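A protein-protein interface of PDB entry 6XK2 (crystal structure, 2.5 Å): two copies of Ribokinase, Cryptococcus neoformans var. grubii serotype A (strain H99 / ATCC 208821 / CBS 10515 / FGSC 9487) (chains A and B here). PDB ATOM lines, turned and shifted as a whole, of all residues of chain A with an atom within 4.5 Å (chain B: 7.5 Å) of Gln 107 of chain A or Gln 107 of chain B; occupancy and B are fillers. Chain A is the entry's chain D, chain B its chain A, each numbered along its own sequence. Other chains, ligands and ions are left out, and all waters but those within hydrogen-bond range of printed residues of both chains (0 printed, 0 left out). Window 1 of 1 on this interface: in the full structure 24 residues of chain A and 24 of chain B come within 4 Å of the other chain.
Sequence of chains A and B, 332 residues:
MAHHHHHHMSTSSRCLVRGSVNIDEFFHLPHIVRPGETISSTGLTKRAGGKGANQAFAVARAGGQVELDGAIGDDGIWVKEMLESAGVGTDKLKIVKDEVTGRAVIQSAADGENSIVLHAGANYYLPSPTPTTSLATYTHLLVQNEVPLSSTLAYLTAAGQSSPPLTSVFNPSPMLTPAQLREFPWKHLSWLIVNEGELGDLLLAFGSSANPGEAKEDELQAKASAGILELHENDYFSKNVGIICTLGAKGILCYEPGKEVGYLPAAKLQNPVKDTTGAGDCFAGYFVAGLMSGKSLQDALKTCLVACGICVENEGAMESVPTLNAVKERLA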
ATOM      1  N   PHE A  27      15.478  23.634  16.822  1.00  0.00           N
ATOM      2  CA  PHE A  27      15.246  25.070  16.723  1.00  0.00           C
ATOM      3  C   PHE A  27      13.962  25.375  17.474  1.00  0.00           C
ATOM      4  O   PHE A  27      12.905  24.829  17.146  1.00  0.00           O
ATOM      5  CB  PHE A  27      15.144  25.532  15.270  1.00  0.00           C
ATOM      6  CG  PHE A  27      16.439  25.441  14.507  1.00  0.00           C
ATOM      7  CD1 PHE A  27      17.332  26.500  14.507  1.00  0.00           C
ATOM      8  CD2 PHE A  27      16.766  24.299  13.795  1.00  0.00           C
ATOM      9  CE1 PHE A  27      18.519  26.422  13.811  1.00  0.00           C
ATOM     10  CE2 PHE A  27      17.956  24.222  13.089  1.00  0.00           C
ATOM     11  CZ  PHE A  27      18.831  25.285  13.103  1.00  0.00           C
ATOM     12  N   LEU A  29      10.958  27.622  18.239  1.00  0.00           N
ATOM     13  CA  LEU A  29      10.196  28.532  17.408  1.00  0.00           C
ATOM     14  C   LEU A  29       8.842  28.806  18.036  1.00  0.00           C
ATOM     15  O   LEU A  29       8.305  27.955  18.748  1.00  0.00           O
ATOM     16  CB  LEU A  29       9.987  27.931  16.014  1.00  0.00           C
ATOM     17  CG  LEU A  29      11.215  27.895  15.125  1.00  0.00           C
ATOM     18  CD1 LEU A  29      11.022  26.916  13.986  1.00  0.00           C
ATOM     19  CD2 LEU A  29      11.433  29.287  14.583  1.00  0.00           C
ATOM     20  N   ILE A  32       5.456  26.319  13.931  1.00  0.00           N
ATOM     21  CA  ILE A  32       6.098  25.678  12.791  1.00  0.00           C
ATOM     22  C   ILE A  32       6.060  26.631  11.604  1.00  0.00           C
ATOM     23  O   ILE A  32       5.024  27.245  11.317  1.00  0.00           O
ATOM     24  CB  ILE A  32       5.393  24.357  12.467  1.00  0.00           C
ATOM     25  CG1 ILE A  32       5.336  23.463  13.706  1.00  0.00           C
ATOM     26  CG2 ILE A  32       6.095  23.652  11.326  1.00  0.00           C
ATOM     27  CD1 ILE A  32       6.668  22.886  14.124  1.00  0.00           C
ATOM     28  N   VAL A  33       7.195  26.762  10.906  1.00  0.00           N
ATOM     29  CA  VAL A  33       7.304  27.736   9.822  1.00  0.00           C
ATOM     30  C   VAL A  33       6.379  27.344   8.676  1.00  0.00           C
ATOM     31  O   VAL A  33       6.299  26.169   8.286  1.00  0.00           O
ATOM     32  CB  VAL A  33       8.765  27.877   9.354  1.00  0.00           C
ATOM     33  CG1 VAL A  33       9.249  26.621   8.670  1.00  0.00           C
ATOM     34  CG2 VAL A  33       8.908  29.073   8.411  1.00  0.00           C
ATOM     35  N   VAL A 105      16.760  18.205  11.364  1.00  0.00           N
ATOM     36  CA  VAL A 105      16.364  19.575  11.656  1.00  0.00           C
ATOM     37  C   VAL A 105      14.974  19.509  12.263  1.00  0.00           C
ATOM     38  O   VAL A 105      13.996  19.241  11.564  1.00  0.00           O
ATOM     39  CB  VAL A 105      16.387  20.449  10.400  1.00  0.00           C
ATOM     40  CG1 VAL A 105      15.862  21.845  10.723  1.00  0.00           C
ATOM     41  CG2 VAL A 105      17.809  20.528   9.818  1.00  0.00           C
ATOM     42  N   ILE A 106      14.881  19.766  13.562  1.00  0.00           N
ATOM     43  CA  ILE A 106      13.643  19.624  14.314  1.00  0.00           C
ATOM     44  C   ILE A 106      13.146  21.013  14.688  1.00  0.00           C
ATOM     45  O   ILE A 106      13.898  21.817  15.256  1.00  0.00           O
ATOM     46  CB  ILE A 106      13.851  18.750  15.560  1.00  0.00           C
ATOM     47  CG1 ILE A 106      14.431  17.396  15.143  1.00  0.00           C
ATOM     48  CG2 ILE A 106      12.543  18.557  16.302  1.00  0.00           C
ATOM     49  CD1 ILE A 106      15.341  16.797  16.164  1.00  0.00           C
ATOM     50  N   GLN A 107      11.893  21.308  14.344  1.00  0.00           N
ATOM     51  CA  GLN A 107      11.253  22.548  14.773  1.00  0.00           C
ATOM     52  C   GLN A 107      10.456  22.260  16.037  1.00  0.00           C
ATOM     53  O   GLN A 107       9.424  21.586  15.989  1.00  0.00           O
ATOM     54  CB  GLN A 107      10.355  23.126  13.682  1.00  0.00           C
ATOM     55  CG  GLN A 107      11.045  23.386  12.357  1.00  0.00           C
ATOM     56  CD  GLN A 107      10.106  23.972  11.328  1.00  0.00           C
ATOM     57  OE1 GLN A 107       9.465  24.985  11.568  1.00  0.00           O
ATOM     58  NE2 GLN A 107       9.998  23.315  10.182  1.00  0.00           N
ATOM     59  N   SER A 108      10.942  22.776  17.164  1.00  0.00           N
ATOM     60  CA  SER A 108      10.269  22.644  18.453  1.00  0.00           C
ATOM     61  C   SER A 108       9.390  23.874  18.688  1.00  0.00           C
ATOM     62  O   SER A 108       9.858  24.906  19.176  1.00  0.00           O
ATOM     63  CB  SER A 108      11.313  22.473  19.550  1.00  0.00           C
ATOM     64  OG  SER A 108      10.703  22.397  20.819  1.00  0.00           O
ATOM     65  N   ALA A 109       8.104  23.762  18.356  1.00  0.00           N
ATOM     66  CA  ALA A 109       7.198  24.897  18.463  1.00  0.00           C
ATOM     67  C   ALA A 109       6.652  25.053  19.879  1.00  0.00           C
ATOM     68  O   ALA A 109       6.505  24.080  20.625  1.00  0.00           O
ATOM     69  CB  ALA A 109       6.050  24.760  17.466  1.00  0.00           C
ATOM     70  N   GLU A 113       3.527  21.411  18.928  1.00  0.00           N
ATOM     71  CA  GLU A 113       3.670  20.652  17.699  1.00  0.00           C
ATOM     72  C   GLU A 113       5.116  20.680  17.225  1.00  0.00           C
ATOM     73  O   GLU A 113       5.784  21.714  17.284  1.00  0.00           O
ATOM     74  CB  GLU A 113       2.744  21.238  16.629  1.00  0.00           C
ATOM     75  CG  GLU A 113       2.326  20.226  15.592  1.00  0.00           C
ATOM     76  CD  GLU A 113       1.967  18.904  16.215  1.00  0.00           C
ATOM     77  OE1 GLU A 113       0.991  18.859  16.990  1.00  0.00           O
ATOM     78  OE2 GLU A 113       2.677  17.915  15.950  1.00  0.00           O
ATOM     79  N   ASN A 114       5.595  19.539  16.738  1.00  0.00           N
ATOM     80  CA  ASN A 114       6.957  19.420  16.234  1.00  0.00           C
ATOM     81  C   ASN A 114       6.934  18.963  14.782  1.00  0.00           C
ATOM     82  O   ASN A 114       5.954  18.385  14.306  1.00  0.00           O
ATOM     83  CB  ASN A 114       7.809  18.469  17.092  1.00  0.00           C
ATOM     84  CG  ASN A 114       8.301  19.117  18.388  1.00  0.00           C
ATOM     85  OD1 ASN A 114       9.407  18.836  18.853  1.00  0.00           O
ATOM     86  ND2 ASN A 114       7.492  20.005  18.959  1.00  0.00           N
ATOM     87  N   SER A 115       8.006  19.292  14.072  1.00  0.00           N
ATOM     88  CA  SER A 115       8.193  18.925  12.678  1.00  0.00           C
ATOM     89  C   SER A 115       9.667  18.631  12.478  1.00  0.00           C
ATOM     90  O   SER A 115      10.519  19.368  12.984  1.00  0.00           O
ATOM     91  CB  SER A 115       7.747  20.044  11.733  1.00  0.00           C
ATOM     92  OG  SER A 115       6.340  20.221  11.765  1.00  0.00           O
ATOM     93  N   VAL A 117      12.858  17.444   9.704  1.00  0.00           N
ATOM     94  CA  VAL A 117      13.432  17.253   8.378  1.00  0.00           C
ATOM     95  C   VAL A 117      14.660  16.368   8.545  1.00  0.00           C
ATOM     96  O   VAL A 117      15.571  16.714   9.307  1.00  0.00           O
ATOM     97  CB  VAL A 117      13.820  18.590   7.721  1.00  0.00           C
ATOM     98  CG1 VAL A 117      14.543  18.342   6.412  1.00  0.00           C
ATOM     99  CG2 VAL A 117      12.589  19.475   7.504  1.00  0.00           C
ATOM    100  N   GLU B  25      21.570  27.192   4.510  1.00  0.00           N
ATOM    101  CA  GLU B  25      21.463  25.765   4.248  1.00  0.00           C
ATOM    102  C   GLU B  25      20.135  25.513   3.552  1.00  0.00           C
ATOM    103  O   GLU B  25      19.073  25.606   4.178  1.00  0.00           O
ATOM    104  CB  GLU B  25      21.585  24.983   5.549  1.00  0.00           C
ATOM    105  CG  GLU B  25      23.031  24.789   5.975  1.00  0.00           C
ATOM    106  CD  GLU B  25      23.167  24.164   7.357  1.00  0.00           C
ATOM    107  OE1 GLU B  25      22.219  24.328   8.159  1.00  0.00           O
ATOM    108  OE2 GLU B  25      24.226  23.546   7.654  1.00  0.00           O
ATOM    109  N   PHE B  26      20.203  25.184   2.259  1.00  0.00           N
ATOM    110  CA  PHE B  26      19.027  24.845   1.461  1.00  0.00           C
ATOM    111  C   PHE B  26      18.801  23.331   1.507  1.00  0.00           C
ATOM    112  O   PHE B  26      19.535  22.563   0.874  1.00  0.00           O
ATOM    113  CB  PHE B  26      19.196  25.308   0.014  1.00  0.00           C
ATOM    114  CG  PHE B  26      19.181  26.786  -0.161  1.00  0.00           C
ATOM    115  CD1 PHE B  26      17.988  27.455  -0.357  1.00  0.00           C
ATOM    116  CD2 PHE B  26      20.359  27.514  -0.144  1.00  0.00           C
ATOM    117  CE1 PHE B  26      17.965  28.832  -0.518  1.00  0.00           C
ATOM    118  CE2 PHE B  26      20.347  28.891  -0.302  1.00  0.00           C
ATOM    119  CZ  PHE B  26      19.150  29.552  -0.491  1.00  0.00           C
ATOM    120  N   PHE B  27      17.741  22.909   2.197  1.00  0.00           N
ATOM    121  CA  PHE B  27      17.318  21.516   2.209  1.00  0.00           C
ATOM    122  C   PHE B  27      16.261  21.340   1.137  1.00  0.00           C
ATOM    123  O   PHE B  27      15.176  21.922   1.224  1.00  0.00           O
ATOM    124  CB  PHE B  27      16.762  21.090   3.569  1.00  0.00           C
ATOM    125  CG  PHE B  27      17.786  21.052   4.659  1.00  0.00           C
ATOM    126  CD1 PHE B  27      18.461  19.880   4.947  1.00  0.00           C
ATOM    127  CD2 PHE B  27      18.091  22.194   5.378  1.00  0.00           C
ATOM    128  CE1 PHE B  27      19.414  19.840   5.940  1.00  0.00           C
ATOM    129  CE2 PHE B  27      19.040  22.162   6.369  1.00  0.00           C
ATOM    130  CZ  PHE B  27      19.700  20.981   6.656  1.00  0.00           C
ATOM    131  N   HIS B  28      16.572  20.516   0.145  1.00  0.00           N
ATOM    132  CA  HIS B  28      15.656  20.272  -0.954  1.00  0.00           C
ATOM    133  C   HIS B  28      14.634  19.232  -0.517  1.00  0.00           C
ATOM    134  O   HIS B  28      14.997  18.122  -0.122  1.00  0.00           O
ATOM    135  CB  HIS B  28      16.444  19.848  -2.189  1.00  0.00           C
ATOM    136  CG  HIS B  28      17.425  20.894  -2.629  1.00  0.00           C
ATOM    137  ND1 HIS B  28      17.055  22.005  -3.362  1.00  0.00           N
ATOM    138  CD2 HIS B  28      18.760  21.011  -2.420  1.00  0.00           C
ATOM    139  CE1 HIS B  28      18.120  22.760  -3.580  1.00  0.00           C
ATOM    140  NE2 HIS B  28      19.166  22.183  -3.016  1.00  0.00           N
ATOM    141  N   LEU B  29      13.361  19.618  -0.532  1.00  0.00           N
ATOM    142  CA  LEU B  29      12.260  18.819  -0.026  1.00  0.00           C
ATOM    143  C   LEU B  29      11.143  18.744  -1.055  1.00  0.00           C
ATOM    144  O   LEU B  29      10.997  19.644  -1.888  1.00  0.00           O
ATOM    145  CB  LEU B  29      11.715  19.418   1.279  1.00  0.00           C
ATOM    146  CG  LEU B  29      12.542  19.217   2.545  1.00  0.00           C
ATOM    147  CD1 LEU B  29      12.097  20.184   3.655  1.00  0.00           C
ATOM    148  CD2 LEU B  29      12.402  17.771   3.010  1.00  0.00           C
ATOM    149  N   HIS B  31       7.909  19.074  -0.302  1.00  0.00           N
ATOM    150  CA  HIS B  31       7.047  20.182   0.074  1.00  0.00           C
ATOM    151  C   HIS B  31       7.514  20.716   1.418  1.00  0.00           C
ATOM    152  O   HIS B  31       8.318  20.088   2.108  1.00  0.00           O
ATOM    153  CB  HIS B  31       5.574  19.772   0.122  1.00  0.00           C
ATOM    154  CG  HIS B  31       5.268  18.682   1.106  1.00  0.00           C
ATOM    155  ND1 HIS B  31       5.341  17.343   0.782  1.00  0.00           N
ATOM    156  CD2 HIS B  31       4.887  18.734   2.405  1.00  0.00           C
ATOM    157  CE1 HIS B  31       5.010  16.618   1.835  1.00  0.00           C
ATOM    158  NE2 HIS B  31       4.735  17.438   2.835  1.00  0.00           N
ATOM    159  N   ILE B  32       7.035  21.912   1.769  1.00  0.00           N
ATOM    160  CA  ILE B  32       7.346  22.467   3.080  1.00  0.00           C
ATOM    161  C   ILE B  32       6.769  21.546   4.141  1.00  0.00           C
ATOM    162  O   ILE B  32       5.615  21.109   4.036  1.00  0.00           O
ATOM    163  CB  ILE B  32       6.786  23.891   3.204  1.00  0.00           C
ATOM    164  CG1 ILE B  32       7.269  24.763   2.042  1.00  0.00           C
ATOM    165  CG2 ILE B  32       7.184  24.505   4.540  1.00  0.00           C
ATOM    166  CD1 ILE B  32       8.746  24.995   2.029  1.00  0.00           C
ATOM    167  N   VAL B  33       7.573  21.214   5.154  1.00  0.00           N
ATOM    168  CA  VAL B  33       7.111  20.261   6.158  1.00  0.00           C
ATOM    169  C   VAL B  33       5.967  20.882   6.947  1.00  0.00           C
ATOM    170  O   VAL B  33       6.023  22.053   7.348  1.00  0.00           O
ATOM    171  CB  VAL B  33       8.266  19.794   7.066  1.00  0.00           C
ATOM    172  CG1 VAL B  33       8.806  20.902   7.951  1.00  0.00           C
ATOM    173  CG2 VAL B  33       7.823  18.601   7.912  1.00  0.00           C
ATOM    174  N   ARG B  34       4.921  20.135   7.115  1.00  0.00           N
ATOM    175  CA  ARG B  34       3.696  20.482   7.818  1.00  0.00           C
ATOM    176  C   ARG B  34       3.797  20.063   9.285  1.00  0.00           C
ATOM    177  O   ARG B  34       4.530  19.124   9.622  1.00  0.00           O
ATOM    178  CB  ARG B  34       2.495  19.804   7.157  1.00  0.00           C
ATOM    179  N   PRO B  35       3.099  20.762  10.182  1.00  0.00           N
ATOM    180  CA  PRO B  35       3.209  20.451  11.617  1.00  0.00           C
ATOM    181  C   PRO B  35       2.876  18.994  11.905  1.00  0.00           C
ATOM    182  O   PRO B  35       1.830  18.489  11.494  1.00  0.00           O
ATOM    183  CB  PRO B  35       2.184  21.390  12.261  1.00  0.00           C
ATOM    184  CG  PRO B  35       2.000  22.502  11.279  1.00  0.00           C
ATOM    185  CD  PRO B  35       2.196  21.899   9.921  1.00  0.00           C
ATOM    186  N   GLY B  36       3.775  18.324  12.636  1.00  0.00           N
ATOM    187  CA  GLY B  36       3.619  16.921  12.973  1.00  0.00           C
ATOM    188  C   GLY B  36       4.233  15.944  11.992  1.00  0.00           C
ATOM    189  O   GLY B  36       4.332  14.752  12.310  1.00  0.00           O
ATOM    190  N   GLU B  37       4.666  16.413  10.827  1.00  0.00           N
ATOM    191  CA  GLU B  37       5.164  15.561   9.760  1.00  0.00           C
ATOM    192  C   GLU B  37       6.672  15.392   9.881  1.00  0.00           C
ATOM    193  O   GLU B  37       7.384  16.284  10.354  1.00  0.00           O
ATOM    194  CB  GLU B  37       4.814  16.165   8.394  1.00  0.00           C
ATOM    195  CG  GLU B  37       5.231  15.364   7.157  1.00  0.00           C
ATOM    196  CD  GLU B  37       4.918  16.117   5.863  1.00  0.00           C
ATOM    197  OE1 GLU B  37       4.752  15.480   4.802  1.00  0.00           O
ATOM    198  OE2 GLU B  37       4.839  17.357   5.903  1.00  0.00           O
ATOM    199  N   ILE B  39       9.855  14.355   7.242  1.00  0.00           N
ATOM    200  CA  ILE B  39      10.110  14.259   5.816  1.00  0.00           C
ATOM    201  C   ILE B  39      11.617  14.274   5.599  1.00  0.00           C
ATOM    202  O   ILE B  39      12.371  14.861   6.382  1.00  0.00           O
ATOM    203  CB  ILE B  39       9.379  15.392   5.058  1.00  0.00           C
ATOM    204  CG1 ILE B  39       9.486  15.198   3.549  1.00  0.00           C
ATOM    205  CG2 ILE B  39       9.901  16.759   5.479  1.00  0.00           C
ATOM    206  CD1 ILE B  39       8.822  16.311   2.768  1.00  0.00           C
ATOM    207  N   ALA B 104      20.618  30.452   8.177  1.00  0.00           N
ATOM    208  CA  ALA B 104      19.269  30.301   7.662  1.00  0.00           C
ATOM    209  C   ALA B 104      19.083  28.832   7.291  1.00  0.00           C
ATOM    210  O   ALA B 104      19.843  28.291   6.471  1.00  0.00           O
ATOM    211  CB  ALA B 104      19.037  31.212   6.460  1.00  0.00           C
ATOM    212  N   VAL B 105      18.111  28.181   7.929  1.00  0.00           N
ATOM    213  CA  VAL B 105      17.684  26.845   7.537  1.00  0.00           C
ATOM    214  C   VAL B 105      16.493  27.020   6.603  1.00  0.00           C
ATOM    215  O   VAL B 105      15.399  27.402   7.035  1.00  0.00           O
ATOM    216  CB  VAL B 105      17.322  25.989   8.756  1.00  0.00           C
ATOM    217  CG1 VAL B 105      16.908  24.573   8.313  1.00  0.00           C
ATOM    218  CG2 VAL B 105      18.501  25.937   9.726  1.00  0.00           C
ATOM    219  N   ILE B 106      16.697  26.741   5.321  1.00  0.00           N
ATOM    220  CA  ILE B 106      15.710  27.039   4.296  1.00  0.00           C
ATOM    221  C   ILE B 106      15.196  25.735   3.712  1.00  0.00           C
ATOM    222  O   ILE B 106      15.973  24.925   3.191  1.00  0.00           O
ATOM    223  CB  ILE B 106      16.289  27.946   3.201  1.00  0.00           C
ATOM    224  CG1 ILE B 106      16.892  29.207   3.834  1.00  0.00           C
ATOM    225  CG2 ILE B 106      15.214  28.285   2.185  1.00  0.00           C
ATOM    226  CD1 ILE B 106      18.212  29.643   3.236  1.00  0.00           C
ATOM    227  N   GLN B 107      13.884  25.549   3.781  1.00  0.00           N
ATOM    228  CA  GLN B 107      13.216  24.473   3.072  1.00  0.00           C
ATOM    229  C   GLN B 107      12.909  24.968   1.667  1.00  0.00           C
ATOM    230  O   GLN B 107      12.083  25.865   1.489  1.00  0.00           O
ATOM    231  CB  GLN B 107      11.935  24.054   3.785  1.00  0.00           C
ATOM    232  CG  GLN B 107      12.105  23.626   5.220  1.00  0.00           C
ATOM    233  CD  GLN B 107      10.779  23.274   5.852  1.00  0.00           C
ATOM    234  OE1 GLN B 107      10.040  22.437   5.341  1.00  0.00           O
ATOM    235  NE2 GLN B 107      10.469  23.911   6.970  1.00  0.00           N
ATOM    236  N   SER B 108      13.567  24.376   0.673  1.00  0.00           N
ATOM    237  CA  SER B 108      13.355  24.697  -0.734  1.00  0.00           C
ATOM    238  C   SER B 108      12.502  23.581  -1.324  1.00  0.00           C
ATOM    239  O   SER B 108      12.999  22.489  -1.624  1.00  0.00           O
ATOM    240  CB  SER B 108      14.694  24.836  -1.454  1.00  0.00           C
ATOM    241  OG  SER B 108      14.529  25.166  -2.824  1.00  0.00           O
ATOM    242  N   ALA B 109      11.212  23.848  -1.483  1.00  0.00           N
ATOM    243  CA  ALA B 109      10.307  22.791  -1.901  1.00  0.00           C
ATOM    244  C   ALA B 109      10.336  22.636  -3.413  1.00  0.00           C
ATOM    245  O   ALA B 109      10.602  23.590  -4.151  1.00  0.00           O
ATOM    246  CB  ALA B 109       8.879  23.085  -1.443  1.00  0.00           C
ATOM    247  N   ALA B 110      10.055  21.414  -3.877  1.00  0.00           N
ATOM    248  CA  ALA B 110       9.954  21.203  -5.314  1.00  0.00           C
ATOM    249  C   ALA B 110       8.755  21.956  -5.868  1.00  0.00           C
ATOM    250  O   ALA B 110       8.774  22.417  -7.013  1.00  0.00           O
ATOM    251  CB  ALA B 110       9.854  19.713  -5.632  1.00  0.00           C
ATOM    252  N   GLY B 112       8.114  24.958  -5.104  1.00  0.00           N
ATOM    253  CA  GLY B 112       8.687  26.238  -5.513  1.00  0.00           C
ATOM    254  C   GLY B 112       8.812  27.190  -4.343  1.00  0.00           C
ATOM    255  O   GLY B 112       9.730  28.017  -4.284  1.00  0.00           O
ATOM    256  N   GLU B 113       7.882  27.062  -3.398  1.00  0.00           N
ATOM    257  CA  GLU B 113       7.873  27.904  -2.212  1.00  0.00           C
ATOM    258  C   GLU B 113       9.068  27.571  -1.328  1.00  0.00           C
ATOM    259  O   GLU B 113       9.553  26.436  -1.302  1.00  0.00           O
ATOM    260  CB  GLU B 113       6.568  27.728  -1.432  1.00  0.00           C
ATOM    261  N   ASN B 114       9.552  28.579  -0.610  1.00  0.00           N
ATOM    262  CA  ASN B 114      10.639  28.407   0.343  1.00  0.00           C
ATOM    263  C   ASN B 114      10.158  28.814   1.729  1.00  0.00           C
ATOM    264  O   ASN B 114       9.170  29.535   1.874  1.00  0.00           O
ATOM    265  CB  ASN B 114      11.888  29.200  -0.050  1.00  0.00           C
ATOM    266  CG  ASN B 114      12.726  28.485  -1.106  1.00  0.00           C
ATOM    267  OD1 ASN B 114      13.950  28.605  -1.134  1.00  0.00           O
ATOM    268  ND2 ASN B 114      12.063  27.748  -1.991  1.00  0.00           N
ATOM    269  N   SER B 115      10.796  28.255   2.746  1.00  0.00           N
ATOM    270  CA  SER B 115      10.546  28.628   4.130  1.00  0.00           C
ATOM    271  C   SER B 115      11.880  28.767   4.839  1.00  0.00           C
ATOM    272  O   SER B 115      12.797  27.969   4.619  1.00  0.00           O
ATOM    273  CB  SER B 115       9.674  27.609   4.839  1.00  0.00           C
ATOM    274  OG  SER B 115       8.337  27.770   4.430  1.00  0.00           O
ATOM    275  N   ILE B 116      11.998  29.789   5.678  1.00  0.00           N
ATOM    276  CA  ILE B 116      13.284  30.149   6.250  1.00  0.00           C
ATOM    277  C   ILE B 116      13.156  30.209   7.759  1.00  0.00           C
ATOM    278  O   ILE B 116      12.242  30.855   8.282  1.00  0.00           O
ATOM    279  CB  ILE B 116      13.795  31.487   5.683  1.00  0.00           C
ATOM    280  CG1 ILE B 116      13.924  31.374   4.163  1.00  0.00           C
ATOM    281  CG2 ILE B 116      15.122  31.855   6.309  1.00  0.00           C
ATOM    282  CD1 ILE B 116      14.341  32.634   3.472  1.00  0.00           C
ATOM    283  N   VAL B 117      14.061  29.523   8.452  1.00  0.00           N
ATOM    284  CA  VAL B 117      14.248  29.663   9.889  1.00  0.00           C
ATOM    285  C   VAL B 117      15.610  30.304  10.095  1.00  0.00           C
ATOM    286  O   VAL B 117      16.624  29.790   9.611  1.00  0.00           O
ATOM    287  CB  VAL B 117      14.161  28.319  10.619  1.00  0.00           C
ATOM    288  CG1 VAL B 117      14.576  28.499  12.081  1.00  0.00           C
ATOM    289  CG2 VAL B 117      12.761  27.747  10.507  1.00  0.00           C
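Gln 107 of chain A touches just these residues of chain B: Val 33 and Gln 107. Of the printed residues of chain B, Glu 113 of chain A touches Pro 35 (3.5 Å) and Gly 36 (3.3 Å). Of the printed residues of chain B, Asn 114 of chain A touches Pro 35 and Gly 36. Of the printed residues of chain B, Ser 115 of chain A touches Arg 34, Pro 35, Gly 36 and Glu 37. His 28 of chain B touches none of the printed residues of chain A. Printed residues of chain A within 4 Å of Val 105 of chain B: Phe 27 (3.5 Å) and Val 105 (3.8 Å). Gln 107 of chain B touches two residues of chain A. The nearest residue of chain B that does not touch Gln 107 of chain A is Val 117 of chain B (4.4 Å). The nearest printed residue of chain A that does not touch Gln 107 of chain B is Val 117 of chain A (4.5 Å).
The backbone carbonyl oxygen of Arg 34 of chain B sits at hydrogen-bond distance from the side-chain hydroxyl of Ser 115 of chain A (3.0 Å). The backbone NH (N) of Gly 36 of chain B sits at hydrogen-bond distance from the backbone carbonyl oxygen (O) of Asn 114 of chain A (2.7 Å). The side-chain hydroxyl of Ser 115 of chain A sits at hydrogen-bond distance from the backbone NH of Gly 36 of chain B (3.3 Å). NE2 of Gln 107 of chain A sits close to NE2 of Gln 107 of chain B (3.3 Å).
Of the 26 printed residues of chain B, 13 touch a printed residue of chain A. Hydrophobic or aromatic side chains of chain A within 4 Å of the printed part of chain B: Phe 27, Leu 29, Val 33, Val 105 and Val 117. Among the printed residues, 19 pairs touch across the chains. Among the printed residues, no Asp or Glu carboxylate lies within 4 Å of a Lys or Arg side-chain nitrogen of the other chain.
Among the printed residues, pairs that only touch across the chains: Phe 27 of chain A with Val 105 of chain B (3.5 Å), Leu 29 of chain A with Val 117 of chain B (3.98 Å), Val 33 of chain A with Gln 107 of chain B (3.4 Å), Val 33 of chain A with Ser 115 of chain B (3.9 Å), Val 33 of chain A with Ile 116 of chain B (3.8 Å), Val 105 of chain A with Phe 27 of chain B (3.7 Å), Val 105 of chain A with Val 105 of chain B (3.8 Å), Gln 107 of chain A with Val 33 of chain B (3.5 Å), Glu 113 of chain A with Pro 35 of chain B (3.5 Å), Glu 113 of chain A with Gly 36 of chain B (3.3 Å), Asn 114 of chain A with Pro 35 of chain B (3.95 Å), Ser 115 of chain A with Pro 35 of chain B (3.1 Å), Ser 115 of chain A with Glu 37 of chain B (3.6 Å), Val 117 of chain A with Leu 29 of chain B (3.9 Å) and Val 117 of chain A with Ile 39 of chain B (3.3 Å).
N of Phe 27 of chain B sits at hydrogen-bond distance from O of Ile 106 of chain B (2.9 Å). The backbone carbonyl oxygen (O) of Phe 27 of chain B sits at hydrogen-bond distance from the backbone NH (N) of Ser 108 of chain B. The backbone NH (N) of Leu 29 of chain B sits at hydrogen-bond distance from the backbone carbonyl oxygen (O) of Ser 108 of chain B. O of Leu 29 of chain B lies within hydrogen-bond range of N of Ala 110 of chain B (2.8 Å). The side-chain amide oxygen (OE1) of Gln 107 of chain A is in hydrogen-bond range of the backbone NH (N) of Val 33 of chain A, 3.0 Å away. O of Val 117 of chain A sits at hydrogen-bond distance from N of Val 105 of chain A, at 2.8 Å.
Phe 27 of chain A touches Val 105 of chain B, and with the chains exchanged Val 105 of chain A touches Phe 27 of chain B. Val 33 of chain A touches Gln 107 of chain B, and with the chains exchanged Gln 107 of chain A touches Val 33 of chain B. Val 33 of chain A touches Ser 115 of chain B, but with the chains exchanged Ser 115 of chain A does not touch Val 33 of chain B (4.02 Å). Gln 107 of chain A touches its own counterpart, Gln 107 of chain B. Positions printed for both chains: 27, 29, 32, 33, 105, 106, 107, 108, 109, 113, 114, 115 and 117.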
